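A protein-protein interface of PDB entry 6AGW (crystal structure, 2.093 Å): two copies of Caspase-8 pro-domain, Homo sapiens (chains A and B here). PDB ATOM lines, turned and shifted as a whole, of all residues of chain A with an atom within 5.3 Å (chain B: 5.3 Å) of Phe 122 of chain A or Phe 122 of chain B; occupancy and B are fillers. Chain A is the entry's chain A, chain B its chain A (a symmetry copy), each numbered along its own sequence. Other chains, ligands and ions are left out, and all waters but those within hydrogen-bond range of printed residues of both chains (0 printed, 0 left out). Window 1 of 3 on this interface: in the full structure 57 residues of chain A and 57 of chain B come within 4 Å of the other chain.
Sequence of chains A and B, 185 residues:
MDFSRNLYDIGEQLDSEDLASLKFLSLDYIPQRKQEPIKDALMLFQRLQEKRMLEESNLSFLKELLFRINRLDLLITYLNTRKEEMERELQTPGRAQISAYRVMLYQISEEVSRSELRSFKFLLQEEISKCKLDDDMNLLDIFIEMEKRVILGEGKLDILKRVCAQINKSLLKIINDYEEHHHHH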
ATOM      1  N   ARG A 118      25.038  26.337   4.838  1.00  0.00           N
ATOM      2  CA  ARG A 118      24.387  27.316   3.976  1.00  0.00           C
ATOM      3  C   ARG A 118      25.441  28.122   3.232  1.00  0.00           C
ATOM      4  O   ARG A 118      25.271  28.440   2.050  1.00  0.00           O
ATOM      5  CB  ARG A 118      23.471  28.252   4.759  1.00  0.00           C
ATOM      6  CG  ARG A 118      22.575  29.080   3.831  1.00  0.00           C
ATOM      7  CD  ARG A 118      22.019  30.302   4.537  1.00  0.00           C
ATOM      8  NE  ARG A 118      20.934  29.960   5.443  1.00  0.00           N
ATOM      9  CZ  ARG A 118      20.992  30.093   6.763  1.00  0.00           C
ATOM     10  NH1 ARG A 118      22.095  30.549   7.342  1.00  0.00           N
ATOM     11  NH2 ARG A 118      19.942  29.762   7.504  1.00  0.00           N
ATOM     12  N   SER A 119      26.535  28.430   3.920  1.00  0.00           N
ATOM     13  CA  SER A 119      27.668  29.076   3.271  1.00  0.00           C
ATOM     14  C   SER A 119      28.257  28.175   2.185  1.00  0.00           C
ATOM     15  O   SER A 119      28.622  28.652   1.108  1.00  0.00           O
ATOM     16  CB  SER A 119      28.736  29.451   4.296  1.00  0.00           C
ATOM     17  OG  SER A 119      28.276  30.510   5.121  1.00  0.00           O
ATOM     18  N   PHE A 120      28.339  26.877   2.465  1.00  0.00           N
ATOM     19  CA  PHE A 120      28.819  25.917   1.471  1.00  0.00           C
ATOM     20  C   PHE A 120      27.973  26.042   0.205  1.00  0.00           C
ATOM     21  O   PHE A 120      28.498  26.046  -0.910  1.00  0.00           O
ATOM     22  CB  PHE A 120      28.762  24.483   2.020  1.00  0.00           C
ATOM     23  CG  PHE A 120      29.510  23.472   1.194  1.00  0.00           C
ATOM     24  CD1 PHE A 120      29.053  23.092  -0.060  1.00  0.00           C
ATOM     25  CD2 PHE A 120      30.655  22.871   1.693  1.00  0.00           C
ATOM     26  CE1 PHE A 120      29.741  22.159  -0.815  1.00  0.00           C
ATOM     27  CE2 PHE A 120      31.340  21.927   0.951  1.00  0.00           C
ATOM     28  CZ  PHE A 120      30.885  21.577  -0.315  1.00  0.00           C
ATOM     29  N   LYS A 121      26.660  26.159   0.384  1.00  0.00           N
ATOM     30  CA  LYS A 121      25.763  26.210  -0.761  1.00  0.00           C
ATOM     31  C   LYS A 121      26.044  27.454  -1.605  1.00  0.00           C
ATOM     32  O   LYS A 121      26.224  27.355  -2.827  1.00  0.00           O
ATOM     33  CB  LYS A 121      24.306  26.164  -0.302  1.00  0.00           C
ATOM     34  CG  LYS A 121      23.872  24.759   0.110  1.00  0.00           C
ATOM     35  CD  LYS A 121      22.468  24.724   0.690  1.00  0.00           C
ATOM     36  CE  LYS A 121      22.167  23.357   1.311  1.00  0.00           C
ATOM     37  NZ  LYS A 121      20.998  23.407   2.234  1.00  0.00           N
ATOM     38  N   PHE A 122      26.117  28.612  -0.954  1.00  0.00           N
ATOM     39  CA  PHE A 122      26.359  29.861  -1.667  1.00  0.00           C
ATOM     40  C   PHE A 122      27.728  29.856  -2.322  1.00  0.00           C
ATOM     41  O   PHE A 122      27.887  30.348  -3.423  1.00  0.00           O
ATOM     42  CB  PHE A 122      26.242  31.065  -0.730  1.00  0.00           C
ATOM     43  CG  PHE A 122      24.829  31.392  -0.328  1.00  0.00           C
ATOM     44  CD1 PHE A 122      23.818  31.425  -1.274  1.00  0.00           C
ATOM     45  CD2 PHE A 122      24.516  31.676   0.995  1.00  0.00           C
ATOM     46  CE1 PHE A 122      22.521  31.727  -0.907  1.00  0.00           C
ATOM     47  CE2 PHE A 122      23.217  31.978   1.367  1.00  0.00           C
ATOM     48  CZ  PHE A 122      22.221  32.004   0.415  1.00  0.00           C
ATOM     49  N   LEU A 123      28.718  29.308  -1.634  1.00  0.00           N
ATOM     50  CA  LEU A 123      30.078  29.321  -2.144  1.00  0.00           C
ATOM     51  C   LEU A 123      30.210  28.362  -3.315  1.00  0.00           C
ATOM     52  O   LEU A 123      30.951  28.624  -4.260  1.00  0.00           O
ATOM     53  CB  LEU A 123      31.070  28.964  -1.043  1.00  0.00           C
ATOM     54  CG  LEU A 123      31.250  30.018   0.057  1.00  0.00           C
ATOM     55  CD1 LEU A 123      32.184  29.491   1.148  1.00  0.00           C
ATOM     56  CD2 LEU A 123      31.759  31.361  -0.503  1.00  0.00           C
ATOM     57  N   LEU A 124      29.476  27.255  -3.252  1.00  0.00           N
ATOM     58  CA  LEU A 124      29.535  26.247  -4.301  1.00  0.00           C
ATOM     59  C   LEU A 124      28.951  26.794  -5.588  1.00  0.00           C
ATOM     60  O   LEU A 124      29.551  26.676  -6.652  1.00  0.00           O
ATOM     61  CB  LEU A 124      28.781  24.985  -3.897  1.00  0.00           C
ATOM     62  CG  LEU A 124      28.663  23.929  -5.007  1.00  0.00           C
ATOM     63  CD1 LEU A 124      30.034  23.470  -5.463  1.00  0.00           C
ATOM     64  CD2 LEU A 124      27.818  22.732  -4.563  1.00  0.00           C
ATOM     65  N   GLN A 125      27.778  27.411  -5.471  1.00  0.00           N
ATOM     66  CA  GLN A 125      27.068  27.918  -6.633  1.00  0.00           C
ATOM     67  C   GLN A 125      27.951  28.956  -7.354  1.00  0.00           C
ATOM     68  O   GLN A 125      28.040  28.965  -8.576  1.00  0.00           O
ATOM     69  CB  GLN A 125      25.724  28.521  -6.216  1.00  0.00           C
ATOM     70  CG  GLN A 125      24.546  27.562  -6.275  1.00  0.00           C
ATOM     71  CD  GLN A 125      23.798  27.552  -7.607  1.00  0.00           C
ATOM     72  OE1 GLN A 125      24.301  28.023  -8.630  1.00  0.00           O
ATOM     73  NE2 GLN A 125      22.556  27.056  -7.586  1.00  0.00           N
ATOM     74  N   GLU A 126      28.637  29.786  -6.575  1.00  0.00           N
ATOM     75  CA  GLU A 126      29.515  30.808  -7.133  1.00  0.00           C
ATOM     76  C   GLU A 126      30.653  30.225  -7.946  1.00  0.00           C
ATOM     77  O   GLU A 126      31.020  30.771  -8.989  1.00  0.00           O
ATOM     78  CB  GLU A 126      30.110  31.693  -6.029  1.00  0.00           C
ATOM     79  CG  GLU A 126      30.961  32.817  -6.628  1.00  0.00           C
ATOM     80  CD  GLU A 126      31.738  33.618  -5.607  1.00  0.00           C
ATOM     81  OE1 GLU A 126      31.396  33.557  -4.409  1.00  0.00           O
ATOM     82  OE2 GLU A 126      32.700  34.306  -6.014  1.00  0.00           O
ATOM     83  N   LEU A 133      26.950  35.441  -4.204  1.00  0.00           N
ATOM     84  CA  LEU A 133      25.768  35.587  -3.355  1.00  0.00           C
ATOM     85  C   LEU A 133      26.088  35.169  -1.919  1.00  0.00           C
ATOM     86  O   LEU A 133      26.826  34.210  -1.695  1.00  0.00           O
ATOM     87  CB  LEU A 133      24.593  34.741  -3.863  1.00  0.00           C
ATOM     88  CG  LEU A 133      24.048  34.812  -5.291  1.00  0.00           C
ATOM     89  CD1 LEU A 133      22.654  34.218  -5.282  1.00  0.00           C
ATOM     90  CD2 LEU A 133      23.998  36.229  -5.823  1.00  0.00           C
ATOM     91  N   ASP A 134      25.535  35.892  -0.951  1.00  0.00           N
ATOM     92  CA  ASP A 134      25.646  35.493   0.448  1.00  0.00           C
ATOM     93  C   ASP A 134      24.393  35.895   1.214  1.00  0.00           C
ATOM     94  O   ASP A 134      23.540  36.632   0.699  1.00  0.00           O
ATOM     95  CB  ASP A 134      26.890  36.101   1.101  1.00  0.00           C
ATOM     96  CG  ASP A 134      26.913  37.609   1.019  1.00  0.00           C
ATOM     97  OD1 ASP A 134      26.039  38.260   1.631  1.00  0.00           O
ATOM     98  OD2 ASP A 134      27.818  38.143   0.342  1.00  0.00           O
ATOM     99  N   ASP A 135      24.286  35.411   2.443  1.00  0.00           N
ATOM    100  CA  ASP A 135      23.074  35.607   3.223  1.00  0.00           C
ATOM    101  C   ASP A 135      22.795  37.094   3.480  1.00  0.00           C
ATOM    102  O   ASP A 135      21.646  37.489   3.670  1.00  0.00           O
ATOM    103  CB  ASP A 135      23.167  34.842   4.544  1.00  0.00           C
ATOM    104  CG  ASP A 135      21.852  34.192   4.932  1.00  0.00           C
ATOM    105  OD1 ASP A 135      20.991  33.994   4.038  1.00  0.00           O
ATOM    106  OD2 ASP A 135      21.677  33.880   6.132  1.00  0.00           O
ATOM    107  N   ARG B 118      16.029  34.649   0.641  1.00  0.00           N
ATOM    108  CA  ARG B 118      17.015  33.577   0.597  1.00  0.00           C
ATOM    109  C   ARG B 118      16.640  32.581  -0.490  1.00  0.00           C
ATOM    110  O   ARG B 118      17.512  32.068  -1.200  1.00  0.00           O
ATOM    111  CB  ARG B 118      17.144  32.860   1.939  1.00  0.00           C
ATOM    112  CG  ARG B 118      18.370  31.940   1.977  1.00  0.00           C
ATOM    113  CD  ARG B 118      18.256  30.905   3.080  1.00  0.00           C
ATOM    114  NE  ARG B 118      18.518  31.476   4.391  1.00  0.00           N
ATOM    115  CZ  ARG B 118      17.614  31.579   5.357  1.00  0.00           C
ATOM    116  NH1 ARG B 118      16.370  31.162   5.157  1.00  0.00           N
ATOM    117  NH2 ARG B 118      17.956  32.107   6.526  1.00  0.00           N
ATOM    118  N   SER B 119      15.343  32.330  -0.630  1.00  0.00           N
ATOM    119  CA  SER B 119      14.857  31.503  -1.727  1.00  0.00           C
ATOM    120  C   SER B 119      15.170  32.152  -3.075  1.00  0.00           C
ATOM    121  O   SER B 119      15.556  31.466  -4.025  1.00  0.00           O
ATOM    122  CB  SER B 119      13.358  31.248  -1.589  1.00  0.00           C
ATOM    123  OG  SER B 119      13.104  30.388  -0.489  1.00  0.00           O
ATOM    124  N   PHE B 120      15.014  33.471  -3.155  1.00  0.00           N
ATOM    125  CA  PHE B 120      15.354  34.203  -4.375  1.00  0.00           C
ATOM    126  C   PHE B 120      16.807  33.908  -4.746  1.00  0.00           C
ATOM    127  O   PHE B 120      17.127  33.669  -5.912  1.00  0.00           O
ATOM    128  CB  PHE B 120      15.139  35.713  -4.189  1.00  0.00           C
ATOM    129  CG  PHE B 120      15.170  36.506  -5.467  1.00  0.00           C
ATOM    130  CD1 PHE B 120      16.353  36.684  -6.171  1.00  0.00           C
ATOM    131  CD2 PHE B 120      14.017  37.110  -5.944  1.00  0.00           C
ATOM    132  CE1 PHE B 120      16.379  37.418  -7.344  1.00  0.00           C
ATOM    133  CE2 PHE B 120      14.038  37.857  -7.107  1.00  0.00           C
ATOM    134  CZ  PHE B 120      15.225  38.003  -7.816  1.00  0.00           C
ATOM    135  N   LYS B 121      17.682  33.914  -3.744  1.00  0.00           N
ATOM    136  CA  LYS B 121      19.101  33.717  -4.006  1.00  0.00           C
ATOM    137  C   LYS B 121      19.349  32.325  -4.590  1.00  0.00           C
ATOM    138  O   LYS B 121      20.007  32.191  -5.630  1.00  0.00           O
ATOM    139  CB  LYS B 121      19.915  33.942  -2.733  1.00  0.00           C
ATOM    140  CG  LYS B 121      20.073  35.424  -2.400  1.00  0.00           C
ATOM    141  CD  LYS B 121      20.769  35.657  -1.069  1.00  0.00           C
ATOM    142  CE  LYS B 121      20.689  37.130  -0.661  1.00  0.00           C
ATOM    143  NZ  LYS B 121      20.979  37.326   0.788  1.00  0.00           N
ATOM    144  N   PHE B 122      18.796  31.302  -3.945  1.00  0.00           N
ATOM    145  CA  PHE B 122      18.988  29.932  -4.405  1.00  0.00           C
ATOM    146  C   PHE B 122      18.370  29.726  -5.777  1.00  0.00           C
ATOM    147  O   PHE B 122      18.927  29.035  -6.608  1.00  0.00           O
ATOM    148  CB  PHE B 122      18.392  28.926  -3.418  1.00  0.00           C
ATOM    149  CG  PHE B 122      19.186  28.772  -2.149  1.00  0.00           C
ATOM    150  CD1 PHE B 122      20.563  28.636  -2.192  1.00  0.00           C
ATOM    151  CD2 PHE B 122      18.551  28.752  -0.914  1.00  0.00           C
ATOM    152  CE1 PHE B 122      21.293  28.493  -1.028  1.00  0.00           C
ATOM    153  CE2 PHE B 122      19.279  28.610   0.256  1.00  0.00           C
ATOM    154  CZ  PHE B 122      20.649  28.479   0.197  1.00  0.00           C
ATOM    155  N   LEU B 123      17.210  30.323  -6.004  1.00  0.00           N
ATOM    156  CA  LEU B 123      16.503  30.127  -7.258  1.00  0.00           C
ATOM    157  C   LEU B 123      17.223  30.849  -8.385  1.00  0.00           C
ATOM    158  O   LEU B 123      17.252  30.372  -9.517  1.00  0.00           O
ATOM    159  CB  LEU B 123      15.061  30.609  -7.146  1.00  0.00           C
ATOM    160  CG  LEU B 123      14.144  29.761  -6.256  1.00  0.00           C
ATOM    161  CD1 LEU B 123      12.764  30.412  -6.143  1.00  0.00           C
ATOM    162  CD2 LEU B 123      14.029  28.308  -6.758  1.00  0.00           C
ATOM    163  N   LEU B 124      17.814  31.996  -8.063  1.00  0.00           N
ATOM    164  CA  LEU B 124      18.514  32.792  -9.062  1.00  0.00           C
ATOM    165  C   LEU B 124      19.753  32.062  -9.541  1.00  0.00           C
ATOM    166  O   LEU B 124      19.990  31.947 -10.739  1.00  0.00           O
ATOM    167  CB  LEU B 124      18.911  34.153  -8.502  1.00  0.00           C
ATOM    168  CG  LEU B 124      19.788  34.997  -9.440  1.00  0.00           C
ATOM    169  CD1 LEU B 124      19.070  35.274 -10.746  1.00  0.00           C
ATOM    170  CD2 LEU B 124      20.224  36.309  -8.781  1.00  0.00           C
ATOM    171  N   GLN B 125      20.528  31.556  -8.586  1.00  0.00           N
ATOM    172  CA  GLN B 125      21.784  30.897  -8.899  1.00  0.00           C
ATOM    173  C   GLN B 125      21.509  29.690  -9.817  1.00  0.00           C
ATOM    174  O   GLN B 125      22.230  29.455 -10.780  1.00  0.00           O
ATOM    175  CB  GLN B 125      22.498  30.470  -7.613  1.00  0.00           C
ATOM    176  CG  GLN B 125      23.496  31.479  -7.069  1.00  0.00           C
ATOM    177  CD  GLN B 125      24.925  31.299  -7.576  1.00  0.00           C
ATOM    178  OE1 GLN B 125      25.172  30.618  -8.576  1.00  0.00           O
ATOM    179  NE2 GLN B 125      25.890  31.872  -6.848  1.00  0.00           N
ATOM    180  N   GLU B 126      20.429  28.969  -9.532  1.00  0.00           N
ATOM    181  CA  GLU B 126      20.053  27.807 -10.329  1.00  0.00           C
ATOM    182  C   GLU B 126      19.751  28.157 -11.772  1.00  0.00           C
ATOM    183  O   GLU B 126      20.109  27.409 -12.684  1.00  0.00           O
ATOM    184  CB  GLU B 126      18.828  27.098  -9.735  1.00  0.00           C
ATOM    185  CG  GLU B 126      18.493  25.830 -10.526  1.00  0.00           C
ATOM    186  CD  GLU B 126      17.189  25.176 -10.126  1.00  0.00           C
ATOM    187  OE1 GLU B 126      16.680  25.474  -9.027  1.00  0.00           O
ATOM    188  OE2 GLU B 126      16.674  24.363 -10.925  1.00  0.00           O
ATOM    189  N   LEU B 133      19.804  23.959  -5.665  1.00  0.00           N
ATOM    190  CA  LEU B 133      20.146  24.047  -4.246  1.00  0.00           C
ATOM    191  C   LEU B 133      19.003  24.694  -3.462  1.00  0.00           C
ATOM    192  O   LEU B 133      18.361  25.627  -3.945  1.00  0.00           O
ATOM    193  CB  LEU B 133      21.424  24.864  -4.017  1.00  0.00           C
ATOM    194  CG  LEU B 133      22.756  24.574  -4.712  1.00  0.00           C
ATOM    195  CD1 LEU B 133      23.851  25.252  -3.912  1.00  0.00           C
ATOM    196  CD2 LEU B 133      23.043  23.091  -4.820  1.00  0.00           C
ATOM    197  N   ASP B 134      18.751  24.196  -2.257  1.00  0.00           N
ATOM    198  CA  ASP B 134      17.790  24.832  -1.362  1.00  0.00           C
ATOM    199  C   ASP B 134      18.222  24.659   0.088  1.00  0.00           C
ATOM    200  O   ASP B 134      19.154  23.900   0.389  1.00  0.00           O
ATOM    201  CB  ASP B 134      16.382  24.270  -1.571  1.00  0.00           C
ATOM    202  CG  ASP B 134      16.316  22.774  -1.375  1.00  0.00           C
ATOM    203  OD1 ASP B 134      16.543  22.303  -0.239  1.00  0.00           O
ATOM    204  OD2 ASP B 134      16.029  22.068  -2.365  1.00  0.00           O
ATOM    205  N   ASP B 135      17.541  25.363   0.982  1.00  0.00           N
ATOM    206  CA  ASP B 135      17.948  25.392   2.379  1.00  0.00           C
ATOM    207  C   ASP B 135      17.895  23.997   3.018  1.00  0.00           C
ATOM    208  O   ASP B 135      18.620  23.720   3.971  1.00  0.00           O
ATOM    209  CB  ASP B 135      17.074  26.374   3.162  1.00  0.00           C
ATOM    210  CG  ASP B 135      17.868  27.170   4.181  1.00  0.00           C
ATOM    211  OD1 ASP B 135      19.114  27.260   4.038  1.00  0.00           O
ATOM    212  OD2 ASP B 135      17.247  27.703   5.128  1.00  0.00           O
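Arg 118 of chain A touches its own counterpart, Arg 118 of chain B.
Lys 121 of chain A touches Leu 133 of chain B, and with the chains exchanged Leu 133 of chain A touches Lys 121 of chain B.
Lys 121 of chain A touches Asp 135 of chain B, and with the chains exchanged Asp 135 of chain A touches Lys 121 of chain B.
Phe 122 of chain B touches its own counterpart, Phe 122 of chain A.
OD1 of Asp 135 of chain B lies within salt-bridge range of NE of Arg 118 of chain A, at 3.5 Å.
The side-chain amino group (NZ) of Lys 121 of chain A sits at hydrogen-bond distance from the backbone carbonyl oxygen (O) of Asp 134 of chain B, 2.7 Å away.
The side-chain amino group (NZ) of Lys 121 of chain A sits at hydrogen-bond distance from the backbone carbonyl oxygen (O) of Asp 135 of chain B (3.0 Å).
The side-chain amide oxygen (OE1) of Gln 125 of chain B sits close to the side-chain amide oxygen (OE1) of Gln 125 of chain A, at 2.7 Å.
NE2 of Gln 125 of chain A lies close to N of Glu 126 of chain B, 3.5 Å away.
N of Glu 126 of chain A sits close to NE2 of Gln 125 of chain B, at 3.5 Å.
The side-chain amino group (NZ) of Lys 121 of chain B lies within hydrogen-bond range of the backbone carbonyl oxygen (O) of Asp 134 of chain A.
The guanidinium group (NE) of Arg 118 of chain B is in salt-bridge range of the side-chain carboxylate (OD1) of Asp 135 of chain A (3.5 Å).
O of Asp 135 of chain A sits at hydrogen-bond distance from NZ of Lys 121 of chain B (3.0 Å).
The guanidinium group (NE) of Arg 118 of chain A lies close to the guanidinium group (NE) of Arg 118 of chain B (3.0 Å).
Phe 122 of chain A touches two residues of chain B.
Of the printed residues of chain A, Phe 122 of chain B touches Lys 121 and Phe 122.
Of the printed residues of chain B, Leu 133 of chain A touches Lys 121 (3.4 Å) and Gln 125 (3.4 Å).
Printed residues of chain A within 4 Å of Leu 133 of chain B: Lys 121 (3.4 Å) and Gln 125 (3.4 Å).
Printed residues of chain B within 4 Å of Asp 135 of chain A: Arg 118 (3.5 Å) and Lys 121 (3.0 Å).
The nearest residue of chain B that does not touch Phe 122 of chain A is Arg 118 of chain B (4.2 Å).
The guanidinium group (NH1) of Arg 118 of chain A is in salt-bridge range of the side-chain carboxylate (OD2) of Asp 135 of chain A (3.6 Å).
The guanidinium group (NH1) of Arg 118 of chain B is in salt-bridge range of the side-chain carboxylate (OD2) of Asp 135 of chain B (3.6 Å).
Among the printed residues, pairs that only touch across the chains: Lys 121 of chain A with Phe 122 of chain B, Lys 121 of chain A with Leu 133 of chain B, Phe 122 of chain A with Lys 121 of chain B, Phe 122 of chain A with Phe 122 of chain B, Gln 125 of chain A with Leu 133 of chain B, Leu 133 of chain A with Lys 121 of chain B and Leu 133 of chain A with Gln 125 of chain B.
Printed residues of chain A that touch a printed residue of chain B: Arg 118, Lys 121, Phe 122, Gln 125, Glu 126, Leu 133, Asp 134 and Asp 135.
Hydrophobic or aromatic side chains of chain A within 4 Å of the printed part of chain B: Phe 122 and Leu 133.
Printed residues of chain B that touch a printed residue of chain A: Arg 118, Lys 121, Phe 122, Gln 125, Glu 126, Leu 133, Asp 134 and Asp 135.
Hydrophobic or aromatic side chains of chain B that line the printed part of chain A: Phe 122 and Leu 133.
Along chain B the printed residues that touch a printed residue of chain A span positions 118 to 135.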
